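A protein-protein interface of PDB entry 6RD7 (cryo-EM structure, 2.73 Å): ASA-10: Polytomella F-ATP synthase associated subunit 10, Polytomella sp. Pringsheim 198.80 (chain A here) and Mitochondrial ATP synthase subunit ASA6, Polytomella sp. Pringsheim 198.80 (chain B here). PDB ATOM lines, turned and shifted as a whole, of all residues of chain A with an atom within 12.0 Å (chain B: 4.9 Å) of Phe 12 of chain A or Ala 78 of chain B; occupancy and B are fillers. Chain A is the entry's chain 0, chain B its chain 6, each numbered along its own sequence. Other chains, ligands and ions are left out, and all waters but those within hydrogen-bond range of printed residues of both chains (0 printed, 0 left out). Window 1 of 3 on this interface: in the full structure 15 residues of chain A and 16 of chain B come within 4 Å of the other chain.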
ATOM      1  N   ALA A   5      10.656   1.917 -29.043  1.00  0.00           N
ATOM      2  CA  ALA A   5      10.362   2.257 -27.658  1.00  0.00           C
ATOM      3  C   ALA A   5      11.343   3.288 -27.124  1.00  0.00           C
ATOM      4  O   ALA A   5      10.990   4.108 -26.266  1.00  0.00           O
ATOM      5  CB  ALA A   5      10.381   0.997 -26.798  1.00  0.00           C
ATOM      6  N   TYR A   6      12.574   3.273 -27.637  1.00  0.00           N
ATOM      7  CA  TYR A   6      13.571   4.260 -27.239  1.00  0.00           C
ATOM      8  C   TYR A   6      13.180   5.653 -27.712  1.00  0.00           C
ATOM      9  O   TYR A   6      13.433   6.649 -27.027  1.00  0.00           O
ATOM     10  CB  TYR A   6      14.938   3.861 -27.795  1.00  0.00           C
ATOM     11  CG  TYR A   6      15.956   4.970 -27.782  1.00  0.00           C
ATOM     12  CD1 TYR A   6      16.536   5.386 -26.594  1.00  0.00           C
ATOM     13  CD2 TYR A   6      16.342   5.599 -28.956  1.00  0.00           C
ATOM     14  CE1 TYR A   6      17.465   6.398 -26.575  1.00  0.00           C
ATOM     15  CE2 TYR A   6      17.265   6.613 -28.946  1.00  0.00           C
ATOM     16  CZ  TYR A   6      17.826   7.008 -27.754  1.00  0.00           C
ATOM     17  OH  TYR A   6      18.754   8.019 -27.740  1.00  0.00           O
ATOM     18  N   PHE A   7      12.552   5.741 -28.883  1.00  0.00           N
ATOM     19  CA  PHE A   7      12.112   7.039 -29.377  1.00  0.00           C
ATOM     20  C   PHE A   7      10.761   7.416 -28.798  1.00  0.00           C
ATOM     21  O   PHE A   7      10.397   8.596 -28.771  1.00  0.00           O
ATOM     22  CB  PHE A   7      12.073   7.034 -30.900  1.00  0.00           C
ATOM     23  CG  PHE A   7      13.420   7.121 -31.512  1.00  0.00           C
ATOM     24  CD1 PHE A   7      14.245   8.189 -31.220  1.00  0.00           C
ATOM     25  CD2 PHE A   7      13.884   6.126 -32.342  1.00  0.00           C
ATOM     26  CE1 PHE A   7      15.497   8.270 -31.759  1.00  0.00           C
ATOM     27  CE2 PHE A   7      15.136   6.202 -32.882  1.00  0.00           C
ATOM     28  CZ  PHE A   7      15.942   7.272 -32.586  1.00  0.00           C
ATOM     29  N   ALA A   8      10.004   6.428 -28.321  1.00  0.00           N
ATOM     30  CA  ALA A   8       8.776   6.734 -27.601  1.00  0.00           C
ATOM     31  C   ALA A   8       9.068   7.226 -26.192  1.00  0.00           C
ATOM     32  O   ALA A   8       8.216   7.874 -25.577  1.00  0.00           O
ATOM     33  CB  ALA A   8       7.871   5.508 -27.564  1.00  0.00           C
ATOM     34  N   LYS A   9      10.256   6.915 -25.660  1.00  0.00           N
ATOM     35  CA  LYS A   9      10.631   7.405 -24.335  1.00  0.00           C
ATOM     36  C   LYS A   9      10.805   8.917 -24.321  1.00  0.00           C
ATOM     37  O   LYS A   9      10.466   9.577 -23.333  1.00  0.00           O
ATOM     38  CB  LYS A   9      11.923   6.744 -23.867  1.00  0.00           C
ATOM     39  CG  LYS A   9      11.764   5.357 -23.309  1.00  0.00           C
ATOM     40  CD  LYS A   9      13.124   4.775 -23.002  1.00  0.00           C
ATOM     41  CE  LYS A   9      13.143   3.286 -23.227  1.00  0.00           C
ATOM     42  NZ  LYS A   9      13.253   2.526 -21.956  1.00  0.00           N
ATOM     43  N   ALA A  10      11.349   9.480 -25.394  1.00  0.00           N
ATOM     44  CA  ALA A  10      11.563  10.917 -25.451  1.00  0.00           C
ATOM     45  C   ALA A  10      10.240  11.633 -25.679  1.00  0.00           C
ATOM     46  O   ALA A  10       9.489  11.297 -26.600  1.00  0.00           O
ATOM     47  CB  ALA A  10      12.554  11.263 -26.560  1.00  0.00           C
ATOM     48  N   GLY A  11       9.953  12.619 -24.838  1.00  0.00           N
ATOM     49  CA  GLY A  11       8.713  13.350 -24.954  1.00  0.00           C
ATOM     50  C   GLY A  11       8.739  14.378 -26.063  1.00  0.00           C
ATOM     51  O   GLY A  11       9.608  14.382 -26.935  1.00  0.00           O
ATOM     52  N   PHE A  12       7.741  15.255 -26.037  1.00  0.00           N
ATOM     53  CA  PHE A  12       7.752  16.406 -26.923  1.00  0.00           C
ATOM     54  C   PHE A  12       8.880  17.344 -26.522  1.00  0.00           C
ATOM     55  O   PHE A  12       9.142  17.557 -25.337  1.00  0.00           O
ATOM     56  CB  PHE A  12       6.411  17.139 -26.872  1.00  0.00           C
ATOM     57  CG  PHE A  12       6.389  18.429 -27.644  1.00  0.00           C
ATOM     58  CD1 PHE A  12       6.225  18.423 -29.016  1.00  0.00           C
ATOM     59  CD2 PHE A  12       6.521  19.649 -26.997  1.00  0.00           C
ATOM     60  CE1 PHE A  12       6.206  19.603 -29.727  1.00  0.00           C
ATOM     61  CE2 PHE A  12       6.513  20.824 -27.705  1.00  0.00           C
ATOM     62  CZ  PHE A  12       6.348  20.803 -29.069  1.00  0.00           C
ATOM     63  N   GLN A  13       9.547  17.906 -27.518  1.00  0.00           N
ATOM     64  CA  GLN A  13      10.614  18.858 -27.284  1.00  0.00           C
ATOM     65  C   GLN A  13      10.504  19.988 -28.293  1.00  0.00           C
ATOM     66  O   GLN A  13      10.206  19.767 -29.468  1.00  0.00           O
ATOM     67  CB  GLN A  13      11.986  18.185 -27.373  1.00  0.00           C
ATOM     68  CG  GLN A  13      13.097  18.960 -26.700  1.00  0.00           C
ATOM     69  CD  GLN A  13      14.286  18.093 -26.354  1.00  0.00           C
ATOM     70  OE1 GLN A  13      14.336  16.918 -26.713  1.00  0.00           O
ATOM     71  NE2 GLN A  13      15.251  18.668 -25.648  1.00  0.00           N
ATOM     72  N   PHE A  14      10.731  21.191 -27.820  1.00  0.00           N
ATOM     73  CA  PHE A  14      10.791  22.373 -28.659  1.00  0.00           C
ATOM     74  C   PHE A  14      12.049  22.340 -29.515  1.00  0.00           C
ATOM     75  O   PHE A  14      12.984  21.588 -29.223  1.00  0.00           O
ATOM     76  CB  PHE A  14      10.783  23.624 -27.784  1.00  0.00           C
ATOM     77  CG  PHE A  14       9.435  23.969 -27.235  1.00  0.00           C
ATOM     78  CD1 PHE A  14       8.324  24.005 -28.059  1.00  0.00           C
ATOM     79  CD2 PHE A  14       9.279  24.265 -25.894  1.00  0.00           C
ATOM     80  CE1 PHE A  14       7.084  24.327 -27.552  1.00  0.00           C
ATOM     81  CE2 PHE A  14       8.043  24.584 -25.382  1.00  0.00           C
ATOM     82  CZ  PHE A  14       6.947  24.618 -26.211  1.00  0.00           C
ATOM     83  N   PRO A  15      12.095  23.112 -30.604  1.00  0.00           N
ATOM     84  CA  PRO A  15      13.364  23.302 -31.314  1.00  0.00           C
ATOM     85  C   PRO A  15      14.403  23.962 -30.418  1.00  0.00           C
ATOM     86  O   PRO A  15      14.067  24.670 -29.468  1.00  0.00           O
ATOM     87  CB  PRO A  15      12.973  24.193 -32.493  1.00  0.00           C
ATOM     88  CG  PRO A  15      11.567  23.842 -32.748  1.00  0.00           C
ATOM     89  CD  PRO A  15      10.958  23.600 -31.404  1.00  0.00           C
ATOM     90  N   ALA A  16      15.676  23.725 -30.742  1.00  0.00           N
ATOM     91  CA  ALA A  16      16.758  23.845 -29.768  1.00  0.00           C
ATOM     92  C   ALA A  16      17.011  25.270 -29.294  1.00  0.00           C
ATOM     93  O   ALA A  16      17.453  25.488 -28.161  1.00  0.00           O
ATOM     94  CB  ALA A  16      18.036  23.258 -30.358  1.00  0.00           C
ATOM     95  N   GLY A  17      16.736  26.253 -30.134  1.00  0.00           N
ATOM     96  CA  GLY A  17      16.934  27.621 -29.714  1.00  0.00           C
ATOM     97  C   GLY A  17      15.667  28.434 -29.792  1.00  0.00           C
ATOM     98  O   GLY A  17      15.709  29.616 -30.136  1.00  0.00           O
ATOM     99  N   LEU A  18      14.530  27.808 -29.479  1.00  0.00           N
ATOM    100  CA  LEU A  18      13.247  28.491 -29.593  1.00  0.00           C
ATOM    101  C   LEU A  18      13.082  29.557 -28.523  1.00  0.00           C
ATOM    102  O   LEU A  18      12.336  30.524 -28.717  1.00  0.00           O
ATOM    103  CB  LEU A  18      12.109  27.480 -29.512  1.00  0.00           C
ATOM    104  CG  LEU A  18      10.754  27.956 -30.027  1.00  0.00           C
ATOM    105  CD1 LEU A  18      10.758  28.035 -31.538  1.00  0.00           C
ATOM    106  CD2 LEU A  18       9.657  27.046 -29.539  1.00  0.00           C
ATOM    107  N   SER A  19      13.774  29.402 -27.393  1.00  0.00           N
ATOM    108  CA  SER A  19      13.751  30.429 -26.362  1.00  0.00           C
ATOM    109  C   SER A  19      14.402  31.716 -26.845  1.00  0.00           C
ATOM    110  O   SER A  19      13.939  32.802 -26.495  1.00  0.00           O
ATOM    111  CB  SER A  19      14.441  29.923 -25.099  1.00  0.00           C
ATOM    112  OG  SER A  19      15.848  30.013 -25.216  1.00  0.00           O
ATOM    113  N   VAL A  22      11.736  33.351 -29.220  1.00  0.00           N
ATOM    114  CA  VAL A  22      10.670  33.947 -28.420  1.00  0.00           C
ATOM    115  C   VAL A  22      11.179  35.185 -27.691  1.00  0.00           C
ATOM    116  O   VAL A  22      10.510  36.223 -27.664  1.00  0.00           O
ATOM    117  CB  VAL A  22      10.091  32.897 -27.452  1.00  0.00           C
ATOM    118  CG1 VAL A  22       9.185  33.535 -26.416  1.00  0.00           C
ATOM    119  CG2 VAL A  22       9.325  31.845 -28.227  1.00  0.00           C
ATOM    120  N   SER B  72       4.954  15.923 -20.987  1.00  0.00           N
ATOM    121  CA  SER B  72       6.183  16.557 -20.537  1.00  0.00           C
ATOM    122  C   SER B  72       5.925  18.014 -20.174  1.00  0.00           C
ATOM    123  O   SER B  72       4.907  18.600 -20.548  1.00  0.00           O
ATOM    124  CB  SER B  72       7.251  16.479 -21.625  1.00  0.00           C
ATOM    125  OG  SER B  72       7.568  15.135 -21.925  1.00  0.00           O
ATOM    126  N   GLN B  74       7.528  20.479 -21.327  1.00  0.00           N
ATOM    127  CA  GLN B  74       7.547  21.245 -22.564  1.00  0.00           C
ATOM    128  C   GLN B  74       6.289  20.991 -23.380  1.00  0.00           C
ATOM    129  O   GLN B  74       5.809  21.887 -24.073  1.00  0.00           O
ATOM    130  CB  GLN B  74       8.799  20.918 -23.368  1.00  0.00           C
ATOM    131  CG  GLN B  74      10.048  21.550 -22.797  1.00  0.00           C
ATOM    132  CD  GLN B  74      11.303  21.010 -23.425  1.00  0.00           C
ATOM    133  OE1 GLN B  74      11.250  20.099 -24.241  1.00  0.00           O
ATOM    134  NE2 GLN B  74      12.443  21.570 -23.049  1.00  0.00           N
ATOM    135  N   ALA B  75       5.713  19.792 -23.277  1.00  0.00           N
ATOM    136  CA  ALA B  75       4.427  19.544 -23.924  1.00  0.00           C
ATOM    137  C   ALA B  75       3.303  20.279 -23.206  1.00  0.00           C
ATOM    138  O   ALA B  75       2.376  20.795 -23.847  1.00  0.00           O
ATOM    139  CB  ALA B  75       4.141  18.046 -23.973  1.00  0.00           C
ATOM    140  N   LYS B  76       3.377  20.345 -21.874  1.00  0.00           N
ATOM    141  CA  LYS B  76       2.425  21.140 -21.108  1.00  0.00           C
ATOM    142  C   LYS B  76       2.573  22.621 -21.421  1.00  0.00           C
ATOM    143  O   LYS B  76       1.571  23.321 -21.588  1.00  0.00           O
ATOM    144  CB  LYS B  76       2.614  20.902 -19.610  1.00  0.00           C
ATOM    145  CG  LYS B  76       2.116  19.566 -19.101  1.00  0.00           C
ATOM    146  CD  LYS B  76       2.751  19.249 -17.756  1.00  0.00           C
ATOM    147  CE  LYS B  76       2.051  18.094 -17.068  1.00  0.00           C
ATOM    148  NZ  LYS B  76       1.743  16.993 -18.020  1.00  0.00           N
ATOM    149  N   ILE B  77       3.817  23.107 -21.518  1.00  0.00           N
ATOM    150  CA  ILE B  77       4.072  24.499 -21.882  1.00  0.00           C
ATOM    151  C   ILE B  77       3.571  24.783 -23.293  1.00  0.00           C
ATOM    152  O   ILE B  77       2.958  25.825 -23.544  1.00  0.00           O
ATOM    153  CB  ILE B  77       5.573  24.819 -21.718  1.00  0.00           C
ATOM    154  CG1 ILE B  77       5.874  25.232 -20.281  1.00  0.00           C
ATOM    155  CG2 ILE B  77       6.038  25.932 -22.642  1.00  0.00           C
ATOM    156  CD1 ILE B  77       7.343  25.193 -19.945  1.00  0.00           C
ATOM    157  N   ALA B  78       3.740  23.823 -24.206  1.00  0.00           N
ATOM    158  CA  ALA B  78       3.314  23.994 -25.591  1.00  0.00           C
ATOM    159  C   ALA B  78       1.802  24.082 -25.707  1.00  0.00           C
ATOM    160  O   ALA B  78       1.277  24.991 -26.354  1.00  0.00           O
ATOM    161  CB  ALA B  78       3.832  22.841 -26.443  1.00  0.00           C
ATOM    162  N   LEU B  79       1.079  23.157 -25.078  1.00  0.00           N
ATOM    163  CA  LEU B  79      -0.371  23.168 -25.238  1.00  0.00           C
ATOM    164  C   LEU B  79      -1.019  24.258 -24.393  1.00  0.00           C
ATOM    165  O   LEU B  79      -2.035  24.838 -24.795  1.00  0.00           O
ATOM    166  CB  LEU B  79      -0.957  21.795 -24.927  1.00  0.00           C
ATOM    167  CG  LEU B  79      -0.456  20.709 -25.884  1.00  0.00           C
ATOM    168  CD1 LEU B  79      -1.195  19.417 -25.642  1.00  0.00           C
ATOM    169  CD2 LEU B  79      -0.577  21.127 -27.350  1.00  0.00           C
ATOM    170  N   PHE B  80      -0.423  24.592 -23.244  1.00  0.00           N
ATOM    171  CA  PHE B  80      -0.913  25.714 -22.457  1.00  0.00           C
ATOM    172  C   PHE B  80      -0.677  27.032 -23.181  1.00  0.00           C
ATOM    173  O   PHE B  80      -1.545  27.907 -23.181  1.00  0.00           O
ATOM    174  CB  PHE B  80      -0.242  25.724 -21.082  1.00  0.00           C
ATOM    175  CG  PHE B  80      -0.397  27.020 -20.340  1.00  0.00           C
ATOM    176  CD1 PHE B  80       0.678  27.887 -20.192  1.00  0.00           C
ATOM    177  CD2 PHE B  80      -1.618  27.374 -19.788  1.00  0.00           C
ATOM    178  CE1 PHE B  80       0.535  29.085 -19.514  1.00  0.00           C
ATOM    179  CE2 PHE B  80      -1.768  28.569 -19.105  1.00  0.00           C
ATOM    180  CZ  PHE B  80      -0.691  29.425 -18.969  1.00  0.00           C
ATOM    181  N   GLY B  81       0.475  27.175 -23.841  1.00  0.00           N
ATOM    182  CA  GLY B  81       0.741  28.387 -24.592  1.00  0.00           C
ATOM    183  C   GLY B  81      -0.070  28.469 -25.867  1.00  0.00           C
ATOM    184  O   GLY B  81      -0.443  29.557 -26.299  1.00  0.00           O
ATOM    185  N   ALA B  82      -0.388  27.319 -26.464  1.00  0.00           N
ATOM    186  CA  ALA B  82      -1.240  27.312 -27.646  1.00  0.00           C
ATOM    187  C   ALA B  82      -2.672  27.678 -27.294  1.00  0.00           C
ATOM    188  O   ALA B  82      -3.315  28.450 -28.011  1.00  0.00           O
ATOM    189  CB  ALA B  82      -1.186  25.946 -28.324  1.00  0.00           C
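The backbone carbonyl oxygen (O) of Phe 12 of chain A lies close to the side-chain amide oxygen (OE1) of Gln 74 of chain B.
Among the printed residues, pairs that only touch across the chains: Gly 11 of chain A with Ser 72 of chain B (3.7 Å), Phe 12 of chain A with Ala 75 of chain B (3.7 Å), Phe 12 of chain A with Ala 78 of chain B (3.6 Å), Gln 13 of chain A with Gln 74 of chain B (3.3 Å), Phe 14 of chain A with Gln 74 of chain B (3.7 Å), Phe 14 of chain A with Ile 77 of chain B (3.7 Å) and Phe 14 of chain A with Ala 78 of chain B (3.6 Å).
Of chain B, only Gln 74 (3.5 Å), Ala 75 (3.7 Å) and Ala 78 (3.6 Å) come within 4 Å of Phe 12 of chain A.
Of chain A, only Gly 11 comes within 4 Å of Ser 72 of chain B.
Gln 74 of chain B touches just these residues of chain A: Phe 12 (3.5 Å), Gln 13 (3.3 Å) and Phe 14 (3.7 Å).
Ala 75 of chain B touches one residue of chain A.
Of chain A, only Phe 14 comes within 4 Å of Ile 77 of chain B.
No residue of chain A comes within 4 Å of Leu 79 of chain B.
Of the printed residues of chain B, Gln 13 of chain A touches Gln 74.
Of the printed residues of chain B, Phe 14 of chain A touches Gln 74, Ile 77 and Ala 78.
The nearest residue of chain B that does not touch Phe 12 of chain A is Ser 72 of chain B (4.1 Å).
The nearest residue of chain A that does not touch Ala 78 of chain B is Gln 13 of chain A (7.5 Å).
Printed residues of chain A that touch a printed residue of chain B: Gly 11, Phe 12, Gln 13 and Phe 14.
Hydrophobic or aromatic side chains of chain A within 4 Å of the printed part of chain B: Phe 12 and Phe 14.
Of the 10 printed residues of chain B, 5 touch a printed residue of chain A.
Among the printed residues, 8 pairs touch across the chains.
Among the printed residues, no Asp or Glu carboxylate lies within 4 Å of a Lys or Arg side-chain nitrogen of the other chain.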
